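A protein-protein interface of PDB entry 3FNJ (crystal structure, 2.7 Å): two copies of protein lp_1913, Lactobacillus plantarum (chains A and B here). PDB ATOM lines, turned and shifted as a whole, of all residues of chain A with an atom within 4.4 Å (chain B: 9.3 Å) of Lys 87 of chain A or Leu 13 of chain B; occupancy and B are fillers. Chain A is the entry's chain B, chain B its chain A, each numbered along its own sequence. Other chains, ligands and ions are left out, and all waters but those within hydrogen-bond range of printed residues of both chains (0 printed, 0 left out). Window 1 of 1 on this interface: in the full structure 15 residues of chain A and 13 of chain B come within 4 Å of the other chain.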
ATOM      1  N   TYR A  12     -16.105  -0.271 -34.093  1.00  0.00           N
ATOM      2  CA  TYR A  12     -15.628  -1.632 -34.356  1.00  0.00           C
ATOM      3  C   TYR A  12     -14.360  -1.633 -35.189  1.00  0.00           C
ATOM      4  O   TYR A  12     -13.422  -2.363 -34.884  1.00  0.00           O
ATOM      5  CB  TYR A  12     -16.690  -2.449 -35.101  1.00  0.00           C
ATOM      6  CG  TYR A  12     -16.344  -3.908 -35.260  1.00  0.00           C
ATOM      7  CD1 TYR A  12     -16.600  -4.820 -34.233  1.00  0.00           C
ATOM      8  CD2 TYR A  12     -15.757  -4.383 -36.438  1.00  0.00           C
ATOM      9  CE1 TYR A  12     -16.285  -6.163 -34.377  1.00  0.00           C
ATOM     10  CE2 TYR A  12     -15.436  -5.731 -36.586  1.00  0.00           C
ATOM     11  CZ  TYR A  12     -15.706  -6.615 -35.552  1.00  0.00           C
ATOM     12  OH  TYR A  12     -15.428  -7.965 -35.694  1.00  0.00           O
ATOM     13  N   TYR A  16      -9.123  -2.509 -35.025  1.00  0.00           N
ATOM     14  CA  TYR A  16      -8.086  -3.091 -35.860  1.00  0.00           C
ATOM     15  C   TYR A  16      -7.077  -2.098 -36.402  1.00  0.00           C
ATOM     16  O   TYR A  16      -7.180  -0.888 -36.195  1.00  0.00           O
ATOM     17  CB  TYR A  16      -8.720  -3.837 -37.042  1.00  0.00           C
ATOM     18  CG  TYR A  16      -9.802  -4.816 -36.645  1.00  0.00           C
ATOM     19  CD1 TYR A  16     -11.087  -4.377 -36.336  1.00  0.00           C
ATOM     20  CD2 TYR A  16      -9.517  -6.171 -36.501  1.00  0.00           C
ATOM     21  CE1 TYR A  16     -12.058  -5.265 -35.887  1.00  0.00           C
ATOM     22  CE2 TYR A  16     -10.477  -7.066 -36.051  1.00  0.00           C
ATOM     23  CZ  TYR A  16     -11.739  -6.611 -35.738  1.00  0.00           C
ATOM     24  OH  TYR A  16     -12.656  -7.498 -35.224  1.00  0.00           O
ATOM     25  N   THR A  84     -11.342 -15.047 -30.455  1.00  0.00           N
ATOM     26  CA  THR A  84     -11.625 -13.873 -29.629  1.00  0.00           C
ATOM     27  C   THR A  84     -10.530 -13.482 -28.639  1.00  0.00           C
ATOM     28  O   THR A  84     -10.727 -12.607 -27.795  1.00  0.00           O
ATOM     29  CB  THR A  84     -12.940 -14.053 -28.850  1.00  0.00           C
ATOM     30  OG1 THR A  84     -12.821 -15.183 -27.981  1.00  0.00           O
ATOM     31  CG2 THR A  84     -14.100 -14.259 -29.808  1.00  0.00           C
ATOM     32  N   LEU A  85      -9.371 -14.116 -28.745  1.00  0.00           N
ATOM     33  CA  LEU A  85      -8.275 -13.806 -27.839  1.00  0.00           C
ATOM     34  C   LEU A  85      -7.701 -12.427 -28.133  1.00  0.00           C
ATOM     35  O   LEU A  85      -7.281 -11.721 -27.219  1.00  0.00           O
ATOM     36  CB  LEU A  85      -7.188 -14.866 -27.958  1.00  0.00           C
ATOM     37  CG  LEU A  85      -6.853 -15.631 -26.685  1.00  0.00           C
ATOM     38  CD1 LEU A  85      -8.100 -16.178 -25.978  1.00  0.00           C
ATOM     39  CD2 LEU A  85      -5.926 -16.745 -27.085  1.00  0.00           C
ATOM     40  N   GLY A  86      -7.694 -12.047 -29.408  1.00  0.00           N
ATOM     41  CA  GLY A  86      -7.177 -10.745 -29.794  1.00  0.00           C
ATOM     42  C   GLY A  86      -7.950  -9.635 -29.117  1.00  0.00           C
ATOM     43  O   GLY A  86      -7.355  -8.706 -28.573  1.00  0.00           O
ATOM     44  N   LYS A  87      -9.277  -9.732 -29.146  1.00  0.00           N
ATOM     45  CA  LYS A  87     -10.134  -8.739 -28.517  1.00  0.00           C
ATOM     46  C   LYS A  87     -10.105  -8.835 -26.994  1.00  0.00           C
ATOM     47  O   LYS A  87     -10.237  -7.820 -26.321  1.00  0.00           O
ATOM     48  CB  LYS A  87     -11.577  -8.870 -29.026  1.00  0.00           C
ATOM     49  CG  LYS A  87     -11.825  -8.216 -30.385  1.00  0.00           C
ATOM     50  CD  LYS A  87     -13.287  -8.287 -30.791  1.00  0.00           C
ATOM     51  CE  LYS A  87     -13.532  -9.376 -31.807  1.00  0.00           C
ATOM     52  NZ  LYS A  87     -12.923  -9.058 -33.108  1.00  0.00           N
ATOM     53  N   THR A  88      -9.943 -10.039 -26.448  1.00  0.00           N
ATOM     54  CA  THR A  88      -9.889 -10.193 -24.990  1.00  0.00           C
ATOM     55  C   THR A  88      -8.717  -9.378 -24.446  1.00  0.00           C
ATOM     56  O   THR A  88      -8.852  -8.672 -23.447  1.00  0.00           O
ATOM     57  CB  THR A  88      -9.692 -11.674 -24.549  1.00  0.00           C
ATOM     58  OG1 THR A  88     -10.884 -12.422 -24.805  1.00  0.00           O
ATOM     59  CG2 THR A  88      -9.385 -11.755 -23.055  1.00  0.00           C
ATOM     60  N   ALA A  89      -7.568  -9.489 -25.111  1.00  0.00           N
ATOM     61  CA  ALA A  89      -6.356  -8.764 -24.729  1.00  0.00           C
ATOM     62  C   ALA A  89      -6.547  -7.255 -24.907  1.00  0.00           C
ATOM     63  O   ALA A  89      -6.229  -6.460 -24.017  1.00  0.00           O
ATOM     64  CB  ALA A  89      -5.175  -9.246 -25.581  1.00  0.00           C
ATOM     65  N   LEU A  90      -7.067  -6.879 -26.069  1.00  0.00           N
ATOM     66  CA  LEU A  90      -7.317  -5.486 -26.407  1.00  0.00           C
ATOM     67  C   LEU A  90      -8.096  -4.794 -25.296  1.00  0.00           C
ATOM     68  O   LEU A  90      -7.900  -3.607 -25.030  1.00  0.00           O
ATOM     69  CB  LEU A  90      -8.098  -5.412 -27.719  1.00  0.00           C
ATOM     70  CG  LEU A  90      -7.960  -4.132 -28.533  1.00  0.00           C
ATOM     71  CD1 LEU A  90      -6.493  -3.851 -28.766  1.00  0.00           C
ATOM     72  CD2 LEU A  90      -8.704  -4.281 -29.849  1.00  0.00           C
ATOM     73  N   LEU A  91      -8.979  -5.543 -24.648  1.00  0.00           N
ATOM     74  CA  LEU A  91      -9.773  -5.002 -23.549  1.00  0.00           C
ATOM     75  C   LEU A  91      -8.884  -4.667 -22.337  1.00  0.00           C
ATOM     76  O   LEU A  91      -8.928  -3.545 -21.824  1.00  0.00           O
ATOM     77  CB  LEU A  91     -10.864  -5.996 -23.141  1.00  0.00           C
ATOM     78  CG  LEU A  91     -11.851  -5.586 -22.043  1.00  0.00           C
ATOM     79  CD1 LEU A  91     -12.509  -4.236 -22.326  1.00  0.00           C
ATOM     80  CD2 LEU A  91     -12.882  -6.668 -21.936  1.00  0.00           C
ATOM     81  N   GLU A 102      -5.816  -4.402 -32.902  1.00  0.00           N
ATOM     82  CA  GLU A 102      -5.800  -5.815 -33.253  1.00  0.00           C
ATOM     83  C   GLU A 102      -5.449  -5.951 -34.725  1.00  0.00           C
ATOM     84  O   GLU A 102      -6.072  -5.316 -35.577  1.00  0.00           O
ATOM     85  CB  GLU A 102      -7.155  -6.479 -33.001  1.00  0.00           C
ATOM     86  CG  GLU A 102      -7.014  -7.962 -32.694  1.00  0.00           C
ATOM     87  CD  GLU A 102      -7.939  -8.852 -33.496  1.00  0.00           C
ATOM     88  OE1 GLU A 102      -9.172  -8.782 -33.279  1.00  0.00           O
ATOM     89  OE2 GLU A 102      -7.420  -9.619 -34.344  1.00  0.00           O
ATOM     90  N   LYS B   5     -14.464   1.963 -27.367  1.00  0.00           N
ATOM     91  CA  LYS B   5     -13.826   0.703 -27.711  1.00  0.00           C
ATOM     92  C   LYS B   5     -13.992  -0.300 -26.584  1.00  0.00           C
ATOM     93  O   LYS B   5     -14.210  -1.488 -26.830  1.00  0.00           O
ATOM     94  CB  LYS B   5     -12.332   0.889 -27.968  1.00  0.00           C
ATOM     95  CG  LYS B   5     -11.993   1.730 -29.169  1.00  0.00           C
ATOM     96  CD  LYS B   5     -10.497   1.769 -29.375  1.00  0.00           C
ATOM     97  CE  LYS B   5     -10.122   2.969 -30.220  1.00  0.00           C
ATOM     98  NZ  LYS B   5      -8.717   2.932 -30.694  1.00  0.00           N
ATOM     99  N   ILE B   6     -13.883   0.194 -25.351  1.00  0.00           N
ATOM    100  CA  ILE B   6     -13.984  -0.618 -24.143  1.00  0.00           C
ATOM    101  C   ILE B   6     -15.397  -1.110 -23.934  1.00  0.00           C
ATOM    102  O   ILE B   6     -15.600  -2.249 -23.534  1.00  0.00           O
ATOM    103  CB  ILE B   6     -13.500   0.190 -22.894  1.00  0.00           C
ATOM    104  CG1 ILE B   6     -11.977   0.359 -22.946  1.00  0.00           C
ATOM    105  CG2 ILE B   6     -13.875  -0.518 -21.598  1.00  0.00           C
ATOM    106  CD1 ILE B   6     -11.410   1.224 -21.824  1.00  0.00           C
ATOM    107  N   GLU B   7     -16.372  -0.256 -24.223  1.00  0.00           N
ATOM    108  CA  GLU B   7     -17.782  -0.611 -24.077  1.00  0.00           C
ATOM    109  C   GLU B   7     -18.188  -1.703 -25.089  1.00  0.00           C
ATOM    110  O   GLU B   7     -18.922  -2.629 -24.743  1.00  0.00           O
ATOM    111  CB  GLU B   7     -18.647   0.638 -24.275  1.00  0.00           C
ATOM    112  CG  GLU B   7     -20.105   0.477 -23.887  1.00  0.00           C
ATOM    113  CD  GLU B   7     -20.293   0.406 -22.386  1.00  0.00           C
ATOM    114  OE1 GLU B   7     -19.864   1.354 -21.688  1.00  0.00           O
ATOM    115  OE2 GLU B   7     -20.875  -0.588 -21.899  1.00  0.00           O
ATOM    116  N   LEU B   8     -17.706  -1.588 -26.331  1.00  0.00           N
ATOM    117  CA  LEU B   8     -18.010  -2.563 -27.371  1.00  0.00           C
ATOM    118  C   LEU B   8     -17.369  -3.910 -27.052  1.00  0.00           C
ATOM    119  O   LEU B   8     -18.036  -4.942 -27.062  1.00  0.00           O
ATOM    120  CB  LEU B   8     -17.515  -2.076 -28.740  1.00  0.00           C
ATOM    121  CG  LEU B   8     -17.657  -3.063 -29.924  1.00  0.00           C
ATOM    122  CD1 LEU B   8     -19.133  -3.393 -30.143  1.00  0.00           C
ATOM    123  CD2 LEU B   8     -17.053  -2.479 -31.185  1.00  0.00           C
ATOM    124  N   LEU B   9     -16.070  -3.890 -26.776  1.00  0.00           N
ATOM    125  CA  LEU B   9     -15.324  -5.096 -26.441  1.00  0.00           C
ATOM    126  C   LEU B   9     -15.910  -5.838 -25.258  1.00  0.00           C
ATOM    127  O   LEU B   9     -15.899  -7.065 -25.218  1.00  0.00           O
ATOM    128  CB  LEU B   9     -13.880  -4.745 -26.114  1.00  0.00           C
ATOM    129  CG  LEU B   9     -12.948  -4.516 -27.286  1.00  0.00           C
ATOM    130  CD1 LEU B   9     -11.704  -3.856 -26.773  1.00  0.00           C
ATOM    131  CD2 LEU B   9     -12.647  -5.827 -27.966  1.00  0.00           C
ATOM    132  N   THR B  10     -16.401  -5.092 -24.279  1.00  0.00           N
ATOM    133  CA  THR B  10     -16.981  -5.707 -23.102  1.00  0.00           C
ATOM    134  C   THR B  10     -18.273  -6.394 -23.453  1.00  0.00           C
ATOM    135  O   THR B  10     -18.484  -7.532 -23.033  1.00  0.00           O
ATOM    136  CB  THR B  10     -17.302  -4.698 -22.008  1.00  0.00           C
ATOM    137  OG1 THR B  10     -16.094  -4.093 -21.545  1.00  0.00           O
ATOM    138  CG2 THR B  10     -17.985  -5.386 -20.859  1.00  0.00           C
ATOM    139  N   THR B  11     -19.147  -5.721 -24.205  1.00  0.00           N
ATOM    140  CA  THR B  11     -20.423  -6.339 -24.570  1.00  0.00           C
ATOM    141  C   THR B  11     -20.149  -7.463 -25.544  1.00  0.00           C
ATOM    142  O   THR B  11     -20.612  -8.579 -25.343  1.00  0.00           O
ATOM    143  CB  THR B  11     -21.408  -5.356 -25.247  1.00  0.00           C
ATOM    144  OG1 THR B  11     -21.641  -4.211 -24.406  1.00  0.00           O
ATOM    145  CG2 THR B  11     -22.733  -6.068 -25.505  1.00  0.00           C
ATOM    146  N   TYR B  12     -19.374  -7.168 -26.587  1.00  0.00           N
ATOM    147  CA  TYR B  12     -19.041  -8.169 -27.599  1.00  0.00           C
ATOM    148  C   TYR B  12     -18.509  -9.450 -26.973  1.00  0.00           C
ATOM    149  O   TYR B  12     -19.020 -10.534 -27.241  1.00  0.00           O
ATOM    150  CB  TYR B  12     -18.003  -7.625 -28.582  1.00  0.00           C
ATOM    151  CG  TYR B  12     -17.877  -8.434 -29.851  1.00  0.00           C
ATOM    152  CD1 TYR B  12     -18.823  -8.310 -30.873  1.00  0.00           C
ATOM    153  CD2 TYR B  12     -16.800  -9.302 -30.048  1.00  0.00           C
ATOM    154  CE1 TYR B  12     -18.696  -9.022 -32.061  1.00  0.00           C
ATOM    155  CE2 TYR B  12     -16.667 -10.021 -31.232  1.00  0.00           C
ATOM    156  CZ  TYR B  12     -17.613  -9.876 -32.238  1.00  0.00           C
ATOM    157  OH  TYR B  12     -17.477 -10.571 -33.426  1.00  0.00           O
ATOM    158  N   LEU B  13     -17.481  -9.326 -26.141  1.00  0.00           N
ATOM    159  CA  LEU B  13     -16.903 -10.495 -25.492  1.00  0.00           C
ATOM    160  C   LEU B  13     -17.914 -11.241 -24.610  1.00  0.00           C
ATOM    161  O   LEU B  13     -17.816 -12.449 -24.445  1.00  0.00           O
ATOM    162  CB  LEU B  13     -15.666 -10.090 -24.682  1.00  0.00           C
ATOM    163  CG  LEU B  13     -14.518  -9.628 -25.575  1.00  0.00           C
ATOM    164  CD1 LEU B  13     -13.389  -9.101 -24.747  1.00  0.00           C
ATOM    165  CD2 LEU B  13     -14.053 -10.789 -26.446  1.00  0.00           C
ATOM    166  N   SER B  14     -18.887 -10.536 -24.054  1.00  0.00           N
ATOM    167  CA  SER B  14     -19.863 -11.212 -23.232  1.00  0.00           C
ATOM    168  C   SER B  14     -20.736 -12.146 -24.068  1.00  0.00           C
ATOM    169  O   SER B  14     -21.498 -12.937 -23.517  1.00  0.00           O
ATOM    170  CB  SER B  14     -20.744 -10.208 -22.483  1.00  0.00           C
ATOM    171  OG  SER B  14     -21.772  -9.684 -23.304  1.00  0.00           O
ATOM    172  N   LEU B  15     -20.640 -12.075 -25.393  1.00  0.00           N
ATOM    173  CA  LEU B  15     -21.458 -12.955 -26.238  1.00  0.00           C
ATOM    174  C   LEU B  15     -20.841 -14.333 -26.370  1.00  0.00           C
ATOM    175  O   LEU B  15     -21.526 -15.285 -26.710  1.00  0.00           O
ATOM    176  CB  LEU B  15     -21.627 -12.367 -27.640  1.00  0.00           C
ATOM    177  CG  LEU B  15     -22.565 -11.173 -27.842  1.00  0.00           C
ATOM    178  CD1 LEU B  15     -22.443 -10.734 -29.283  1.00  0.00           C
ATOM    179  CD2 LEU B  15     -24.008 -11.541 -27.506  1.00  0.00           C
ATOM    180  N   TYR B  16     -19.546 -14.427 -26.081  1.00  0.00           N
ATOM    181  CA  TYR B  16     -18.796 -15.670 -26.193  1.00  0.00           C
ATOM    182  C   TYR B  16     -18.472 -16.378 -24.875  1.00  0.00           C
ATOM    183  O   TYR B  16     -18.545 -15.786 -23.792  1.00  0.00           O
ATOM    184  CB  TYR B  16     -17.478 -15.403 -26.933  1.00  0.00           C
ATOM    185  CG  TYR B  16     -17.633 -15.028 -28.378  1.00  0.00           C
ATOM    186  CD1 TYR B  16     -17.948 -13.723 -28.753  1.00  0.00           C
ATOM    187  CD2 TYR B  16     -17.495 -15.991 -29.378  1.00  0.00           C
ATOM    188  CE1 TYR B  16     -18.125 -13.389 -30.092  1.00  0.00           C
ATOM    189  CE2 TYR B  16     -17.671 -15.670 -30.715  1.00  0.00           C
ATOM    190  CZ  TYR B  16     -17.989 -14.371 -31.073  1.00  0.00           C
ATOM    191  OH  TYR B  16     -18.194 -14.075 -32.409  1.00  0.00           O
ATOM    192  N   ILE B  17     -18.108 -17.657 -25.001  1.00  0.00           N
ATOM    193  CA  ILE B  17     -17.698 -18.491 -23.874  1.00  0.00           C
ATOM    194  C   ILE B  17     -16.442 -19.290 -24.287  1.00  0.00           C
ATOM    195  O   ILE B  17     -16.380 -19.851 -25.378  1.00  0.00           O
ATOM    196  CB  ILE B  17     -18.823 -19.461 -23.420  1.00  0.00           C
ATOM    197  CG1 ILE B  17     -18.451 -20.043 -22.055  1.00  0.00           C
ATOM    198  CG2 ILE B  17     -19.033 -20.581 -24.448  1.00  0.00           C
ATOM    199  CD1 ILE B  17     -19.519 -20.939 -21.429  1.00  0.00           C
ATOM    200  N   ASP B  18     -15.440 -19.311 -23.410  1.00  0.00           N
ATOM    201  CA  ASP B  18     -14.171 -20.000 -23.653  1.00  0.00           C
ATOM    202  C   ASP B  18     -14.384 -21.496 -23.847  1.00  0.00           C
ATOM    203  O   ASP B  18     -15.201 -22.100 -23.156  1.00  0.00           O
ATOM    204  CB  ASP B  18     -13.224 -19.769 -22.465  1.00  0.00           C
ATOM    205  CG  ASP B  18     -11.754 -19.996 -22.817  1.00  0.00           C
ATOM    206  OD1 ASP B  18     -11.428 -21.067 -23.374  1.00  0.00           O
ATOM    207  OD2 ASP B  18     -10.916 -19.113 -22.516  1.00  0.00           O
ATOM    208  N   GLY B  81     -15.623 -18.759 -36.455  1.00  0.00           N
ATOM    209  CA  GLY B  81     -16.345 -17.651 -35.859  1.00  0.00           C
ATOM    210  C   GLY B  81     -16.468 -16.472 -36.799  1.00  0.00           C
ATOM    211  O   GLY B  81     -16.637 -15.329 -36.368  1.00  0.00           O
ATOM    212  N   LYS B  87     -24.250 -15.607 -33.994  1.00  0.00           N
ATOM    213  CA  LYS B  87     -24.913 -14.402 -33.498  1.00  0.00           C
ATOM    214  C   LYS B  87     -26.422 -14.396 -33.748  1.00  0.00           C
ATOM    215  O   LYS B  87     -27.181 -13.873 -32.929  1.00  0.00           O
ATOM    216  CB  LYS B  87     -24.302 -13.162 -34.142  1.00  0.00           C
ATOM    217  CG  LYS B  87     -22.816 -13.033 -33.938  1.00  0.00           C
ATOM    218  CD  LYS B  87     -22.309 -11.733 -34.496  1.00  0.00           C
ATOM    219  CE  LYS B  87     -20.906 -11.530 -34.043  1.00  0.00           C
ATOM    220  NZ  LYS B  87     -20.905 -11.765 -32.593  1.00  0.00           N
ATOM    221  N   LEU B  90     -27.953 -16.757 -31.367  1.00  0.00           N
ATOM    222  CA  LEU B  90     -27.914 -16.141 -30.052  1.00  0.00           C
ATOM    223  C   LEU B  90     -29.051 -15.135 -29.906  1.00  0.00           C
ATOM    224  O   LEU B  90     -29.596 -14.971 -28.817  1.00  0.00           O
ATOM    225  CB  LEU B  90     -26.558 -15.461 -29.839  1.00  0.00           C
ATOM    226  CG  LEU B  90     -25.755 -15.799 -28.581  1.00  0.00           C
ATOM    227  CD1 LEU B  90     -25.554 -17.285 -28.440  1.00  0.00           C
ATOM    228  CD2 LEU B  90     -24.421 -15.100 -28.661  1.00  0.00           C
ATOM    229  N   ALA B 100     -27.499 -18.185 -23.496  1.00  0.00           N
ATOM    230  CA  ALA B 100     -26.540 -18.822 -24.380  1.00  0.00           C
ATOM    231  C   ALA B 100     -25.319 -17.987 -24.688  1.00  0.00           C
ATOM    232  O   ALA B 100     -25.274 -16.786 -24.425  1.00  0.00           O
ATOM    233  CB  ALA B 100     -27.223 -19.218 -25.666  1.00  0.00           C
ATOM    234  N   TYR B 101     -24.327 -18.660 -25.256  1.00  0.00           N
ATOM    235  CA  TYR B 101     -23.066 -18.043 -25.628  1.00  0.00           C
ATOM    236  C   TYR B 101     -22.574 -18.699 -26.911  1.00  0.00           C
ATOM    237  O   TYR B 101     -23.058 -19.761 -27.293  1.00  0.00           O
ATOM    238  CB  TYR B 101     -22.033 -18.271 -24.525  1.00  0.00           C
ATOM    239  CG  TYR B 101     -22.446 -17.772 -23.163  1.00  0.00           C
ATOM    240  CD1 TYR B 101     -22.365 -16.418 -22.839  1.00  0.00           C
ATOM    241  CD2 TYR B 101     -22.909 -18.653 -22.191  1.00  0.00           C
ATOM    242  CE1 TYR B 101     -22.732 -15.957 -21.580  1.00  0.00           C
ATOM    243  CE2 TYR B 101     -23.281 -18.198 -20.934  1.00  0.00           C
ATOM    244  CZ  TYR B 101     -23.189 -16.853 -20.635  1.00  0.00           C
ATOM    245  OH  TYR B 101     -23.550 -16.396 -19.389  1.00  0.00           O
ATOM    246  N   GLU B 102     -21.610 -18.062 -27.572  1.00  0.00           N
ATOM    247  CA  GLU B 102     -21.035 -18.618 -28.790  1.00  0.00           C
ATOM    248  C   GLU B 102     -19.713 -19.288 -28.414  1.00  0.00           C
ATOM    249  O   GLU B 102     -18.947 -18.754 -27.605  1.00  0.00           O
ATOM    250  CB  GLU B 102     -20.780 -17.528 -29.844  1.00  0.00           C
ATOM    251  CG  GLU B 102     -20.444 -18.123 -31.226  1.00  0.00           C
ATOM    252  CD  GLU B 102     -20.182 -17.093 -32.315  1.00  0.00           C
ATOM    253  OE1 GLU B 102     -20.991 -16.153 -32.472  1.00  0.00           O
ATOM    254  OE2 GLU B 102     -19.170 -17.237 -33.037  1.00  0.00           O
ATOM    255  N   ALA B 104     -16.250 -19.766 -28.433  1.00  0.00           N
ATOM    256  CA  ALA B 104     -15.090 -19.021 -28.889  1.00  0.00           C
ATOM    257  C   ALA B 104     -14.157 -19.966 -29.631  1.00  0.00           C
ATOM    258  O   ALA B 104     -13.669 -20.934 -29.058  1.00  0.00           O
ATOM    259  CB  ALA B 104     -14.371 -18.407 -27.692  1.00  0.00           C
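Lys 87 of chain A touches Tyr 12 of chain B, but with the chains exchanged Tyr 12 of chain A does not touch Lys 87 of chain B (6.7 Å).
Positions printed for both chains: 12, 16, 87, 90 and 102.
Of the 11 pairs that touch across the chains among the printed residues, none has its exchanged pair printed and touching as well.
NZ of Lys 87 of chain A lies within hydrogen-bond range of OH of Tyr 16 of chain A (2.6 Å).
The side-chain carboxylate (OE2) of Glu 102 of chain B sits close to the side-chain hydroxyl (OH) of Tyr 16 of chain B (3.4 Å).
O of Ile 17 of chain B is in hydrogen-bond range of N of Ala 104 of chain B, at 3.1 Å.
The side-chain hydroxyl (OH) of Tyr 16 of chain A is in hydrogen-bond range of the side-chain hydroxyl (OH) of Tyr 12 of chain A (2.9 Å).
The side-chain amino group (NZ) of Lys 87 of chain A is in salt-bridge range of the side-chain carboxylate (OE1) of Glu 102 of chain A (3.8 Å).
The side-chain hydroxyl of Thr 10 of chain B lies within hydrogen-bond range of the backbone carbonyl oxygen of Ile 6 of chain B, at 2.8 Å.
CA of Tyr 12 of chain A touches CD2 of Leu 8 of chain B, 3.6 Å away.
Thr 84 of chain A touches Tyr 16 of chain B (CG2 to CD2, 3.8 Å).
Ala 104 of chain B touches Thr 84 of chain A.
CE2 of Tyr 12 of chain B touches CE of Lys 87 of chain A, at 3.3 Å.
Lys 87 of chain A touches Leu 13 of chain B (O to CD1, 3.7 Å).
Thr 88 of chain A touches Leu 13 of chain B (CA to CD1, 3.7 Å).
Leu 91 of chain A touches Ile 6 of chain B.
CD1 of Leu 9 of chain B touches N of Leu 91 of chain A (3.8 Å).
OG1 of Thr 10 of chain B touches CD1 of Leu 91 of chain A, at 3.7 Å.
CD2 of Leu 91 of chain A touches CD1 of Leu 13 of chain B (3.8 Å).
Lys 87 of chain A touches just these residues of chain B: Leu 9 (3.4 Å), Tyr 12 (3.3 Å) and Leu 13 (3.7 Å).
Of the printed residues of chain A, Leu 13 of chain B touches Lys 87 (3.7 Å), Thr 88 (3.7 Å) and Leu 91 (3.8 Å).
Gly 86 of chain A touches none of the printed residues of chain B.
Thr 88 of chain A touches just one residue of chain B: Leu 13 (3.7 Å).
No residue of chain B comes within 4 Å of Ala 89 of chain A.
Of the printed residues of chain A, Leu 8 of chain B touches Tyr 12.
Of the printed residues of chain A, Thr 10 of chain B touches Leu 91 (3.7 Å).
Of the printed residues of chain A, Tyr 12 of chain B touches Lys 87 (3.3 Å).
Of the printed residues of chain A, Ala 104 of chain B touches Thr 84.
Leu 90 of chain B touches none of the printed residues of chain A.
Leu 15 of chain B touches none of the printed residues of chain A.
The nearest residue of chain A that does not touch Leu 13 of chain B is Thr 84 of chain A (4.02 Å).
Of the 11 printed residues of chain A, 5 touch a printed residue of chain B.
Of the 21 printed residues of chain B, 8 touch a printed residue of chain A.
Among the printed residues, no Asp or Glu carboxylate lies within 4 Å of a Lys or Arg side-chain nitrogen of the other chain.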
